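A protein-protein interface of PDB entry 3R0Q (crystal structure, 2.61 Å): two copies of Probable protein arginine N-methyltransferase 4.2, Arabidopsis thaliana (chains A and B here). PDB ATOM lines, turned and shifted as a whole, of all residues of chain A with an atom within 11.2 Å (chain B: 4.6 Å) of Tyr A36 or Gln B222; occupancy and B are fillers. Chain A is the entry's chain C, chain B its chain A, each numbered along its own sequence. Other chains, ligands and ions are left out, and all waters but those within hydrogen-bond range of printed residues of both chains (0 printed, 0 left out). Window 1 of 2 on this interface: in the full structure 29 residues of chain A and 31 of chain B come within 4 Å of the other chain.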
ATOM      1  N   CYS A  30     -19.106 -14.474  -1.245  1.00  0.00           N
ATOM      2  CA  CYS A  30     -19.544 -13.097  -1.456  1.00  0.00           C
ATOM      3  C   CYS A  30     -20.574 -12.938  -2.574  1.00  0.00           C
ATOM      4  O   CYS A  30     -21.697 -12.506  -2.334  1.00  0.00           O
ATOM      5  CB  CYS A  30     -18.338 -12.190  -1.727  1.00  0.00           C
ATOM      6  SG  CYS A  30     -18.755 -10.494  -2.207  1.00  0.00           S
ATOM      7  N   THR A  31     -20.180 -13.274  -3.796  1.00  0.00           N
ATOM      8  CA  THR A  31     -21.028 -13.048  -4.964  1.00  0.00           C
ATOM      9  C   THR A  31     -22.331 -13.844  -4.951  1.00  0.00           C
ATOM     10  O   THR A  31     -23.297 -13.469  -5.613  1.00  0.00           O
ATOM     11  CB  THR A  31     -20.274 -13.346  -6.272  1.00  0.00           C
ATOM     12  OG1 THR A  31     -20.955 -12.725  -7.368  1.00  0.00           O
ATOM     13  CG2 THR A  31     -20.198 -14.845  -6.513  1.00  0.00           C
ATOM     14  N   TYR A  32     -22.357 -14.940  -4.204  1.00  0.00           N
ATOM     15  CA  TYR A  32     -23.529 -15.809  -4.172  1.00  0.00           C
ATOM     16  C   TYR A  32     -24.613 -15.296  -3.229  1.00  0.00           C
ATOM     17  O   TYR A  32     -25.671 -15.908  -3.101  1.00  0.00           O
ATOM     18  CB  TYR A  32     -23.129 -17.233  -3.781  1.00  0.00           C
ATOM     19  CG  TYR A  32     -22.754 -18.110  -4.953  1.00  0.00           C
ATOM     20  CD1 TYR A  32     -23.616 -18.274  -6.027  1.00  0.00           C
ATOM     21  CD2 TYR A  32     -21.537 -18.775  -4.985  1.00  0.00           C
ATOM     22  CE1 TYR A  32     -23.277 -19.074  -7.098  1.00  0.00           C
ATOM     23  CE2 TYR A  32     -21.190 -19.576  -6.051  1.00  0.00           C
ATOM     24  CZ  TYR A  32     -22.063 -19.722  -7.104  1.00  0.00           C
ATOM     25  OH  TYR A  32     -21.720 -20.521  -8.168  1.00  0.00           O
ATOM     26  N   SER A  33     -24.348 -14.173  -2.571  1.00  0.00           N
ATOM     27  CA  SER A  33     -25.300 -13.612  -1.620  1.00  0.00           C
ATOM     28  C   SER A  33     -26.213 -12.568  -2.257  1.00  0.00           C
ATOM     29  O   SER A  33     -27.065 -11.991  -1.585  1.00  0.00           O
ATOM     30  CB  SER A  33     -24.572 -13.016  -0.413  1.00  0.00           C
ATOM     31  OG  SER A  33     -23.407 -12.319  -0.809  1.00  0.00           O
ATOM     32  N   PHE A  34     -26.037 -12.332  -3.551  1.00  0.00           N
ATOM     33  CA  PHE A  34     -26.876 -11.372  -4.271  1.00  0.00           C
ATOM     34  C   PHE A  34     -28.080 -12.041  -4.949  1.00  0.00           C
ATOM     35  O   PHE A  34     -27.929 -13.038  -5.647  1.00  0.00           O
ATOM     36  CB  PHE A  34     -26.045 -10.608  -5.318  1.00  0.00           C
ATOM     37  CG  PHE A  34     -25.049  -9.654  -4.728  1.00  0.00           C
ATOM     38  CD1 PHE A  34     -25.414  -8.346  -4.427  1.00  0.00           C
ATOM     39  CD2 PHE A  34     -23.747 -10.058  -4.468  1.00  0.00           C
ATOM     40  CE1 PHE A  34     -24.487  -7.452  -3.871  1.00  0.00           C
ATOM     41  CE2 PHE A  34     -22.812  -9.166  -3.913  1.00  0.00           C
ATOM     42  CZ  PHE A  34     -23.187  -7.867  -3.609  1.00  0.00           C
ATOM     43  N   LEU A  35     -29.272 -11.487  -4.747  1.00  0.00           N
ATOM     44  CA  LEU A  35     -30.452 -11.908  -5.507  1.00  0.00           C
ATOM     45  C   LEU A  35     -30.144 -11.865  -6.985  1.00  0.00           C
ATOM     46  O   LEU A  35     -30.543 -12.742  -7.746  1.00  0.00           O
ATOM     47  CB  LEU A  35     -31.623 -10.961  -5.267  1.00  0.00           C
ATOM     48  CG  LEU A  35     -32.426 -11.053  -3.972  1.00  0.00           C
ATOM     49  CD1 LEU A  35     -33.129 -12.381  -3.906  1.00  0.00           C
ATOM     50  CD2 LEU A  35     -31.535 -10.859  -2.765  1.00  0.00           C
ATOM     51  N   TYR A  36     -29.434 -10.812  -7.370  1.00  0.00           N
ATOM     52  CA  TYR A  36     -29.129 -10.515  -8.757  1.00  0.00           C
ATOM     53  C   TYR A  36     -28.327 -11.629  -9.401  1.00  0.00           C
ATOM     54  O   TYR A  36     -28.536 -11.960 -10.559  1.00  0.00           O
ATOM     55  CB  TYR A  36     -28.357  -9.196  -8.847  1.00  0.00           C
ATOM     56  CG  TYR A  36     -27.986  -8.838 -10.258  1.00  0.00           C
ATOM     57  CD1 TYR A  36     -28.973  -8.553 -11.199  1.00  0.00           C
ATOM     58  CD2 TYR A  36     -26.659  -8.805 -10.662  1.00  0.00           C
ATOM     59  CE1 TYR A  36     -28.651  -8.242 -12.487  1.00  0.00           C
ATOM     60  CE2 TYR A  36     -26.326  -8.485 -11.957  1.00  0.00           C
ATOM     61  CZ  TYR A  36     -27.328  -8.205 -12.865  1.00  0.00           C
ATOM     62  OH  TYR A  36     -27.000  -7.883 -14.161  1.00  0.00           O
ATOM     63  N   HIS A  37     -27.392 -12.191  -8.648  1.00  0.00           N
ATOM     64  CA  HIS A  37     -26.531 -13.256  -9.150  1.00  0.00           C
ATOM     65  C   HIS A  37     -27.327 -14.542  -9.191  1.00  0.00           C
ATOM     66  O   HIS A  37     -27.216 -15.332 -10.130  1.00  0.00           O
ATOM     67  CB  HIS A  37     -25.321 -13.437  -8.234  1.00  0.00           C
ATOM     68  N   GLN A  38     -28.143 -14.735  -8.162  1.00  0.00           N
ATOM     69  CA  GLN A  38     -28.939 -15.942  -8.028  1.00  0.00           C
ATOM     70  C   GLN A  38     -29.957 -16.078  -9.152  1.00  0.00           C
ATOM     71  O   GLN A  38     -30.203 -17.185  -9.626  1.00  0.00           O
ATOM     72  CB  GLN A  38     -29.621 -15.985  -6.660  1.00  0.00           C
ATOM     73  CG  GLN A  38     -28.645 -16.092  -5.498  1.00  0.00           C
ATOM     74  CD  GLN A  38     -27.968 -17.452  -5.411  1.00  0.00           C
ATOM     75  OE1 GLN A  38     -27.958 -18.217  -6.369  1.00  0.00           O
ATOM     76  NE2 GLN A  38     -27.421 -17.766  -4.246  1.00  0.00           N
ATOM     77  N   LYS A  39     -30.540 -14.962  -9.587  1.00  0.00           N
ATOM     78  CA  LYS A  39     -31.509 -15.007 -10.690  1.00  0.00           C
ATOM     79  C   LYS A  39     -30.823 -15.271 -12.030  1.00  0.00           C
ATOM     80  O   LYS A  39     -31.439 -15.799 -12.956  1.00  0.00           O
ATOM     81  CB  LYS A  39     -32.328 -13.714 -10.786  1.00  0.00           C
ATOM     82  CG  LYS A  39     -31.517 -12.521 -11.227  1.00  0.00           C
ATOM     83  CD  LYS A  39     -32.402 -11.385 -11.741  1.00  0.00           C
ATOM     84  CE  LYS A  39     -32.863 -11.625 -13.176  1.00  0.00           C
ATOM     85  NZ  LYS A  39     -33.454 -10.393 -13.753  1.00  0.00           N
ATOM     86  N   ASP A  40     -29.562 -14.881 -12.144  1.00  0.00           N
ATOM     87  CA  ASP A  40     -28.805 -15.180 -13.347  1.00  0.00           C
ATOM     88  C   ASP A  40     -28.905 -16.684 -13.572  1.00  0.00           C
ATOM     89  O   ASP A  40     -29.350 -17.139 -14.623  1.00  0.00           O
ATOM     90  CB  ASP A  40     -27.339 -14.767 -13.171  1.00  0.00           C
ATOM     91  CG  ASP A  40     -26.969 -13.531 -13.987  1.00  0.00           C
ATOM     92  OD1 ASP A  40     -27.873 -12.951 -14.634  1.00  0.00           O
ATOM     93  OD2 ASP A  40     -25.776 -13.128 -13.959  1.00  0.00           O
ATOM     94  N   MET A  41     -28.512 -17.447 -12.557  1.00  0.00           N
ATOM     95  CA  MET A  41     -28.573 -18.901 -12.611  1.00  0.00           C
ATOM     96  C   MET A  41     -29.979 -19.390 -12.915  1.00  0.00           C
ATOM     97  O   MET A  41     -30.183 -20.223 -13.800  1.00  0.00           O
ATOM     98  CB  MET A  41     -28.124 -19.511 -11.288  1.00  0.00           C
ATOM     99  CG  MET A  41     -26.768 -19.063 -10.829  1.00  0.00           C
ATOM    100  SD  MET A  41     -26.411 -19.769  -9.218  1.00  0.00           S
ATOM    101  CE  MET A  41     -25.411 -21.174  -9.699  1.00  0.00           C
ATOM    102  N   LEU A  42     -30.944 -18.874 -12.167  1.00  0.00           N
ATOM    103  CA  LEU A  42     -32.332 -19.267 -12.338  1.00  0.00           C
ATOM    104  C   LEU A  42     -32.840 -18.938 -13.739  1.00  0.00           C
ATOM    105  O   LEU A  42     -33.861 -19.467 -14.179  1.00  0.00           O
ATOM    106  CB  LEU A  42     -33.205 -18.580 -11.287  1.00  0.00           C
ATOM    107  CG  LEU A  42     -32.971 -18.989  -9.835  1.00  0.00           C
ATOM    108  CD1 LEU A  42     -33.501 -17.933  -8.886  1.00  0.00           C
ATOM    109  CD2 LEU A  42     -33.634 -20.315  -9.567  1.00  0.00           C
ATOM    110  N   SER A  43     -32.127 -18.058 -14.434  1.00  0.00           N
ATOM    111  CA  SER A  43     -32.539 -17.618 -15.763  1.00  0.00           C
ATOM    112  C   SER A  43     -32.121 -18.615 -16.832  1.00  0.00           C
ATOM    113  O   SER A  43     -32.543 -18.526 -17.989  1.00  0.00           O
ATOM    114  CB  SER A  43     -31.940 -16.248 -16.089  1.00  0.00           C
ATOM    115  OG  SER A  43     -32.500 -15.235 -15.273  1.00  0.00           O
ATOM    116  N   ASP A  44     -31.273 -19.558 -16.441  1.00  0.00           N
ATOM    117  CA  ASP A  44     -30.797 -20.547 -17.384  1.00  0.00           C
ATOM    118  C   ASP A  44     -31.875 -21.600 -17.637  1.00  0.00           C
ATOM    119  O   ASP A  44     -32.051 -22.525 -16.845  1.00  0.00           O
ATOM    120  CB  ASP A  44     -29.513 -21.189 -16.874  1.00  0.00           C
ATOM    121  CG  ASP A  44     -28.774 -21.936 -17.958  1.00  0.00           C
ATOM    122  OD1 ASP A  44     -27.690 -22.474 -17.658  1.00  0.00           O
ATOM    123  OD2 ASP A  44     -29.281 -21.980 -19.107  1.00  0.00           O
ATOM    124  N   ARG A  47     -30.179 -25.013 -17.856  1.00  0.00           N
ATOM    125  CA  ARG A  47     -29.883 -25.466 -16.501  1.00  0.00           C
ATOM    126  C   ARG A  47     -31.156 -25.865 -15.749  1.00  0.00           C
ATOM    127  O   ARG A  47     -31.218 -26.938 -15.159  1.00  0.00           O
ATOM    128  CB  ARG A  47     -29.142 -24.378 -15.731  1.00  0.00           C
ATOM    129  CG  ARG A  47     -28.555 -24.841 -14.416  1.00  0.00           C
ATOM    130  CD  ARG A  47     -28.157 -23.649 -13.584  1.00  0.00           C
ATOM    131  NE  ARG A  47     -29.252 -23.242 -12.723  1.00  0.00           N
ATOM    132  CZ  ARG A  47     -29.229 -23.353 -11.401  1.00  0.00           C
ATOM    133  NH1 ARG A  47     -28.142 -23.819 -10.803  1.00  0.00           N
ATOM    134  NH2 ARG A  47     -30.274 -22.976 -10.681  1.00  0.00           N
ATOM    135  N   GLY A  73     -29.156 -21.864  -1.871  1.00  0.00           N
ATOM    136  CA  GLY A  73     -29.261 -20.511  -2.391  1.00  0.00           C
ATOM    137  C   GLY A  73     -30.705 -20.041  -2.334  1.00  0.00           C
ATOM    138  O   GLY A  73     -31.278 -19.938  -1.249  1.00  0.00           O
ATOM    139  N   SER A  74     -31.310 -19.787  -3.491  1.00  0.00           N
ATOM    140  CA  SER A  74     -32.702 -19.350  -3.541  1.00  0.00           C
ATOM    141  C   SER A  74     -33.634 -20.389  -2.939  1.00  0.00           C
ATOM    142  O   SER A  74     -34.784 -20.092  -2.614  1.00  0.00           O
ATOM    143  CB  SER A  74     -33.128 -19.089  -4.981  1.00  0.00           C
ATOM    144  OG  SER A  74     -33.153 -20.295  -5.712  1.00  0.00           O
ATOM    145  N   THR A  95     -24.892 -18.598   3.012  1.00  0.00           N
ATOM    146  CA  THR A  95     -25.003 -17.145   2.928  1.00  0.00           C
ATOM    147  C   THR A  95     -26.315 -16.620   3.525  1.00  0.00           C
ATOM    148  O   THR A  95     -27.203 -17.402   3.894  1.00  0.00           O
ATOM    149  CB  THR A  95     -24.925 -16.680   1.462  1.00  0.00           C
ATOM    150  OG1 THR A  95     -23.868 -17.368   0.788  1.00  0.00           O
ATOM    151  CG2 THR A  95     -24.642 -15.207   1.394  1.00  0.00           C
ATOM    152  N   MET A  97     -28.435 -15.511   1.961  1.00  0.00           N
ATOM    153  CA  MET A  97     -29.418 -15.884   0.962  1.00  0.00           C
ATOM    154  C   MET A  97     -30.397 -16.857   1.604  1.00  0.00           C
ATOM    155  O   MET A  97     -31.508 -17.026   1.131  1.00  0.00           O
ATOM    156  CB  MET A  97     -28.737 -16.550  -0.233  1.00  0.00           C
ATOM    157  CG  MET A  97     -29.633 -16.689  -1.435  1.00  0.00           C
ATOM    158  SD  MET A  97     -29.951 -15.113  -2.261  1.00  0.00           S
ATOM    159  CE  MET A  97     -31.596 -15.443  -2.903  1.00  0.00           C
ATOM    160  N   HIS A 100     -33.776 -15.605   2.326  1.00  0.00           N
ATOM    161  CA  HIS A 100     -34.688 -15.442   1.203  1.00  0.00           C
ATOM    162  C   HIS A 100     -35.302 -16.789   0.827  1.00  0.00           C
ATOM    163  O   HIS A 100     -36.516 -16.911   0.650  1.00  0.00           O
ATOM    164  CB  HIS A 100     -33.956 -14.801   0.022  1.00  0.00           C
ATOM    165  CG  HIS A 100     -33.461 -13.409   0.305  1.00  0.00           C
ATOM    166  ND1 HIS A 100     -34.295 -12.394   0.725  1.00  0.00           N
ATOM    167  CD2 HIS A 100     -32.222 -12.866   0.222  1.00  0.00           C
ATOM    168  CE1 HIS A 100     -33.590 -11.290   0.895  1.00  0.00           C
ATOM    169  NE2 HIS A 100     -32.331 -11.547   0.597  1.00  0.00           N
ATOM    170  N   HIS A 314     -25.098 -20.797 -18.793  1.00  0.00           N
ATOM    171  CA  HIS A 314     -24.351 -19.705 -18.189  1.00  0.00           C
ATOM    172  C   HIS A 314     -22.893 -20.090 -17.984  1.00  0.00           C
ATOM    173  O   HIS A 314     -22.059 -19.243 -17.647  1.00  0.00           O
ATOM    174  CB  HIS A 314     -25.010 -19.222 -16.886  1.00  0.00           C
ATOM    175  CG  HIS A 314     -24.788 -20.117 -15.702  1.00  0.00           C
ATOM    176  ND1 HIS A 314     -25.545 -21.249 -15.465  1.00  0.00           N
ATOM    177  CD2 HIS A 314     -23.933 -20.015 -14.657  1.00  0.00           C
ATOM    178  CE1 HIS A 314     -25.143 -21.819 -14.343  1.00  0.00           C
ATOM    179  NE2 HIS A 314     -24.165 -21.091 -13.833  1.00  0.00           N
ATOM    180  N   PHE B 189     -32.032   1.239 -12.872  1.00  0.00           N
ATOM    181  CA  PHE B 189     -32.811   0.564 -11.862  1.00  0.00           C
ATOM    182  C   PHE B 189     -34.127   0.062 -12.456  1.00  0.00           C
ATOM    183  O   PHE B 189     -34.443  -1.120 -12.347  1.00  0.00           O
ATOM    184  CB  PHE B 189     -33.057   1.488 -10.673  1.00  0.00           C
ATOM    185  CG  PHE B 189     -33.855   0.856  -9.580  1.00  0.00           C
ATOM    186  CD1 PHE B 189     -33.238   0.100  -8.604  1.00  0.00           C
ATOM    187  CD2 PHE B 189     -35.225   1.012  -9.536  1.00  0.00           C
ATOM    188  CE1 PHE B 189     -33.981  -0.493  -7.600  1.00  0.00           C
ATOM    189  CE2 PHE B 189     -35.975   0.427  -8.540  1.00  0.00           C
ATOM    190  CZ  PHE B 189     -35.355  -0.330  -7.570  1.00  0.00           C
ATOM    191  N   ALA B 192     -33.753  -2.893 -14.411  1.00  0.00           N
ATOM    192  CA  ALA B 192     -33.584  -4.017 -13.491  1.00  0.00           C
ATOM    193  C   ALA B 192     -34.926  -4.547 -13.000  1.00  0.00           C
ATOM    194  O   ALA B 192     -35.215  -5.740 -13.125  1.00  0.00           O
ATOM    195  CB  ALA B 192     -32.710  -3.611 -12.309  1.00  0.00           C
ATOM    196  N   PHE B 218     -35.071  -7.888  -3.691  1.00  0.00           N
ATOM    197  CA  PHE B 218     -34.473  -7.663  -4.999  1.00  0.00           C
ATOM    198  C   PHE B 218     -34.372  -6.161  -5.233  1.00  0.00           C
ATOM    199  O   PHE B 218     -33.317  -5.660  -5.617  1.00  0.00           O
ATOM    200  CB  PHE B 218     -35.272  -8.332  -6.132  1.00  0.00           C
ATOM    201  CG  PHE B 218     -34.553  -8.321  -7.451  1.00  0.00           C
ATOM    202  CD1 PHE B 218     -33.524  -9.222  -7.703  1.00  0.00           C
ATOM    203  CD2 PHE B 218     -34.867  -7.383  -8.425  1.00  0.00           C
ATOM    204  CE1 PHE B 218     -32.835  -9.203  -8.907  1.00  0.00           C
ATOM    205  CE2 PHE B 218     -34.187  -7.355  -9.635  1.00  0.00           C
ATOM    206  CZ  PHE B 218     -33.170  -8.268  -9.876  1.00  0.00           C
ATOM    207  N   ALA B 219     -35.468  -5.447  -4.975  1.00  0.00           N
ATOM    208  CA  ALA B 219     -35.524  -4.004  -5.218  1.00  0.00           C
ATOM    209  C   ALA B 219     -34.423  -3.252  -4.476  1.00  0.00           C
ATOM    210  O   ALA B 219     -33.725  -2.429  -5.073  1.00  0.00           O
ATOM    211  CB  ALA B 219     -36.879  -3.450  -4.831  1.00  0.00           C
ATOM    212  N   GLU B 220     -34.275  -3.535  -3.180  1.00  0.00           N
ATOM    213  CA  GLU B 220     -33.341  -2.804  -2.323  1.00  0.00           C
ATOM    214  C   GLU B 220     -31.884  -3.012  -2.748  1.00  0.00           C
ATOM    215  O   GLU B 220     -31.042  -2.119  -2.639  1.00  0.00           O
ATOM    216  CB  GLU B 220     -33.551  -3.214  -0.862  1.00  0.00           C
ATOM    217  CG  GLU B 220     -34.952  -2.877  -0.319  1.00  0.00           C
ATOM    218  CD  GLU B 220     -35.206  -3.450   1.066  1.00  0.00           C
ATOM    219  OE1 GLU B 220     -36.222  -3.067   1.686  1.00  0.00           O
ATOM    220  OE2 GLU B 220     -34.398  -4.284   1.532  1.00  0.00           O
ATOM    221  N   GLU B 221     -31.603  -4.195  -3.231  1.00  0.00           N
ATOM    222  CA  GLU B 221     -30.310  -4.560  -3.697  1.00  0.00           C
ATOM    223  C   GLU B 221     -30.048  -3.741  -4.890  1.00  0.00           C
ATOM    224  O   GLU B 221     -28.967  -3.370  -5.108  1.00  0.00           O
ATOM    225  CB  GLU B 221     -30.299  -6.031  -4.033  1.00  0.00           C
ATOM    226  CG  GLU B 221     -28.972  -6.695  -4.174  1.00  0.00           C
ATOM    227  CD  GLU B 221     -29.114  -8.091  -4.659  1.00  0.00           C
ATOM    228  OE1 GLU B 221     -29.339  -8.301  -5.822  1.00  0.00           O
ATOM    229  OE2 GLU B 221     -28.994  -9.011  -3.883  1.00  0.00           O
ATOM    230  N   GLN B 222     -31.063  -3.416  -5.645  1.00  0.00           N
ATOM    231  CA  GLN B 222     -30.846  -2.747  -6.887  1.00  0.00           C
ATOM    232  C   GLN B 222     -30.778  -1.278  -6.648  1.00  0.00           C
ATOM    233  O   GLN B 222     -30.206  -0.568  -7.415  1.00  0.00           O
ATOM    234  CB  GLN B 222     -31.921  -3.067  -7.916  1.00  0.00           C
ATOM    235  CG  GLN B 222     -32.084  -4.505  -8.397  1.00  0.00           C
ATOM    236  CD  GLN B 222     -30.838  -5.336  -8.517  1.00  0.00           C
ATOM    237  OE1 GLN B 222     -30.739  -6.375  -7.926  1.00  0.00           O
ATOM    238  NE2 GLN B 222     -29.923  -4.908  -9.322  1.00  0.00           N
ATOM    239  N   GLU B 223     -31.343  -0.812  -5.557  1.00  0.00           N
ATOM    240  CA  GLU B 223     -31.225   0.592  -5.250  1.00  0.00           C
ATOM    241  C   GLU B 223     -29.939   0.854  -4.529  1.00  0.00           C
ATOM    242  O   GLU B 223     -29.260   1.818  -4.790  1.00  0.00           O
ATOM    243  CB  GLU B 223     -32.414   1.102  -4.455  1.00  0.00           C
ATOM    244  N   LYS B 224     -29.607  -0.044  -3.630  1.00  0.00           N
ATOM    245  CA  LYS B 224     -28.320   0.011  -2.941  1.00  0.00           C
ATOM    246  C   LYS B 224     -27.150   0.071  -3.931  1.00  0.00           C
ATOM    247  O   LYS B 224     -26.113   0.680  -3.666  1.00  0.00           O
ATOM    248  CB  LYS B 224     -28.160  -1.206  -2.026  1.00  0.00           C
ATOM    249  CG  LYS B 224     -26.770  -1.338  -1.395  1.00  0.00           C
ATOM    250  N   TYR B 225     -27.334  -0.555  -5.083  1.00  0.00           N
ATOM    251  CA  TYR B 225     -26.241  -0.759  -6.026  1.00  0.00           C
ATOM    252  C   TYR B 225     -26.165   0.295  -7.135  1.00  0.00           C
ATOM    253  O   TYR B 225     -25.076   0.674  -7.560  1.00  0.00           O
ATOM    254  CB  TYR B 225     -26.350  -2.162  -6.630  1.00  0.00           C
ATOM    255  CG  TYR B 225     -25.607  -2.321  -7.927  1.00  0.00           C
ATOM    256  CD1 TYR B 225     -24.280  -1.931  -8.034  1.00  0.00           C
ATOM    257  CD2 TYR B 225     -26.218  -2.872  -9.038  1.00  0.00           C
ATOM    258  CE1 TYR B 225     -23.593  -2.065  -9.206  1.00  0.00           C
ATOM    259  CE2 TYR B 225     -25.527  -3.019 -10.221  1.00  0.00           C
ATOM    260  CZ  TYR B 225     -24.216  -2.613 -10.294  1.00  0.00           C
ATOM    261  OH  TYR B 225     -23.513  -2.750 -11.464  1.00  0.00           O
ATOM    262  N   TYR B 226     -27.316   0.756  -7.616  1.00  0.00           N
ATOM    263  CA  TYR B 226     -27.346   1.784  -8.645  1.00  0.00           C
ATOM    264  C   TYR B 226     -27.376   3.190  -8.085  1.00  0.00           C
ATOM    265  O   TYR B 226     -26.851   4.117  -8.709  1.00  0.00           O
ATOM    266  CB  TYR B 226     -28.567   1.622  -9.531  1.00  0.00           C
ATOM    267  CG  TYR B 226     -28.511   0.431 -10.428  1.00  0.00           C
ATOM    268  CD1 TYR B 226     -27.544   0.331 -11.411  1.00  0.00           C
ATOM    269  CD2 TYR B 226     -29.439  -0.588 -10.309  1.00  0.00           C
ATOM    270  CE1 TYR B 226     -27.497  -0.758 -12.239  1.00  0.00           C
ATOM    271  CE2 TYR B 226     -29.404  -1.679 -11.137  1.00  0.00           C
ATOM    272  CZ  TYR B 226     -28.432  -1.760 -12.101  1.00  0.00           C
ATOM    273  OH  TYR B 226     -28.389  -2.853 -12.934  1.00  0.00           O
ATOM    274  N   ILE B 227     -28.007   3.352  -6.926  1.00  0.00           N
ATOM    275  CA  ILE B 227     -28.290   4.681  -6.388  1.00  0.00           C
ATOM    276  C   ILE B 227     -27.330   5.065  -5.241  1.00  0.00           C
ATOM    277  O   ILE B 227     -26.565   6.024  -5.379  1.00  0.00           O
ATOM    278  CB  ILE B 227     -29.744   4.802  -5.866  1.00  0.00           C
ATOM    279  CG1 ILE B 227     -30.750   4.301  -6.905  1.00  0.00           C
ATOM    280  CG2 ILE B 227     -30.047   6.242  -5.482  1.00  0.00           C
ATOM    281  CD1 ILE B 227     -30.958   5.241  -8.094  1.00  0.00           C
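The backbone NH (N) of Tyr A36 lies within hydrogen-bond range of the side-chain carboxylate (OE1) of Glu B221, 3.0 Å away.
N of Leu A35 sits at hydrogen-bond distance from OE2 of Glu B221 (2.6 Å).
The backbone carbonyl oxygen (O) of Lys A39 is in hydrogen-bond range of the side-chain hydroxyl (OG) of Ser A43 (2.6 Å).
The side-chain carboxylate (OE1) of Glu B221 sits close to the side-chain amide oxygen (OE1) of Gln B222 (3.2 Å).
Phe A34 touches Glu B221 (CA to OE2, 3.2 Å).
CD1 of Phe B218 touches CB of Leu A35 (3.5 Å).
Tyr A36 touches Phe B218 (CA to CE1, 3.9 Å).
Tyr A36 touches Gln B222 (CB to OE1, 3.8 Å).
CD of Lys A39 touches CE1 of Phe B218 (3.6 Å).
Of the printed residues of chain B, Tyr A36 touches Phe B218, Glu B221 and Gln B222.
Gln B222 touches one residue of chain A.
No residue of chain A comes within 4 Å of Phe B189.
No residue of chain A comes within 4 Å of Ala B192.
Phe B218 touches three residues of chain A.
Glu B221 touches just these residues of chain A: Phe A34 (3.2 Å), Leu A35 (2.6 Å) and Tyr A36 (3.0 Å).
No residue of chain A comes within 4 Å of Glu B223.
No residue of chain A comes within 4 Å of Lys B224.
No residue of chain A comes within 4 Å of Tyr B225.
No residue of chain A comes within 4 Å of Tyr B226.
Of the printed residues of chain B, Phe A34 touches Glu B221 (3.2 Å).
Printed residues of chain B within 4 Å of Lys A39: Phe B218.
Of the printed residues of chain B, Leu A35 touches Phe B218 and Glu B221.
The nearest residue of chain A that does not touch Gln B222 is Leu A35 (5.4 Å).
Of the 22 printed residues of chain A, 4 touch a printed residue of chain B.
Printed residues of chain A that touch a printed residue of chain B: Phe A34, Leu A35, Tyr A36 and Lys A39.
Hydrophobic or aromatic side chains of chain A that line the printed part of chain B: Phe A34, Leu A35 and Tyr A36.
Hydrophobic or aromatic side chains of chain B that line the printed part of chain A: Phe B218.
Among the printed residues, 7 pairs touch across the chains.
Among the printed residues, no Asp or Glu carboxylate lies within 4 Å of a Lys or Arg side-chain nitrogen of the other chain.
No position is printed for both chains.
Of the 7 pairs that touch across the chains among the printed residues, none has its exchanged pair printed and touching as well.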
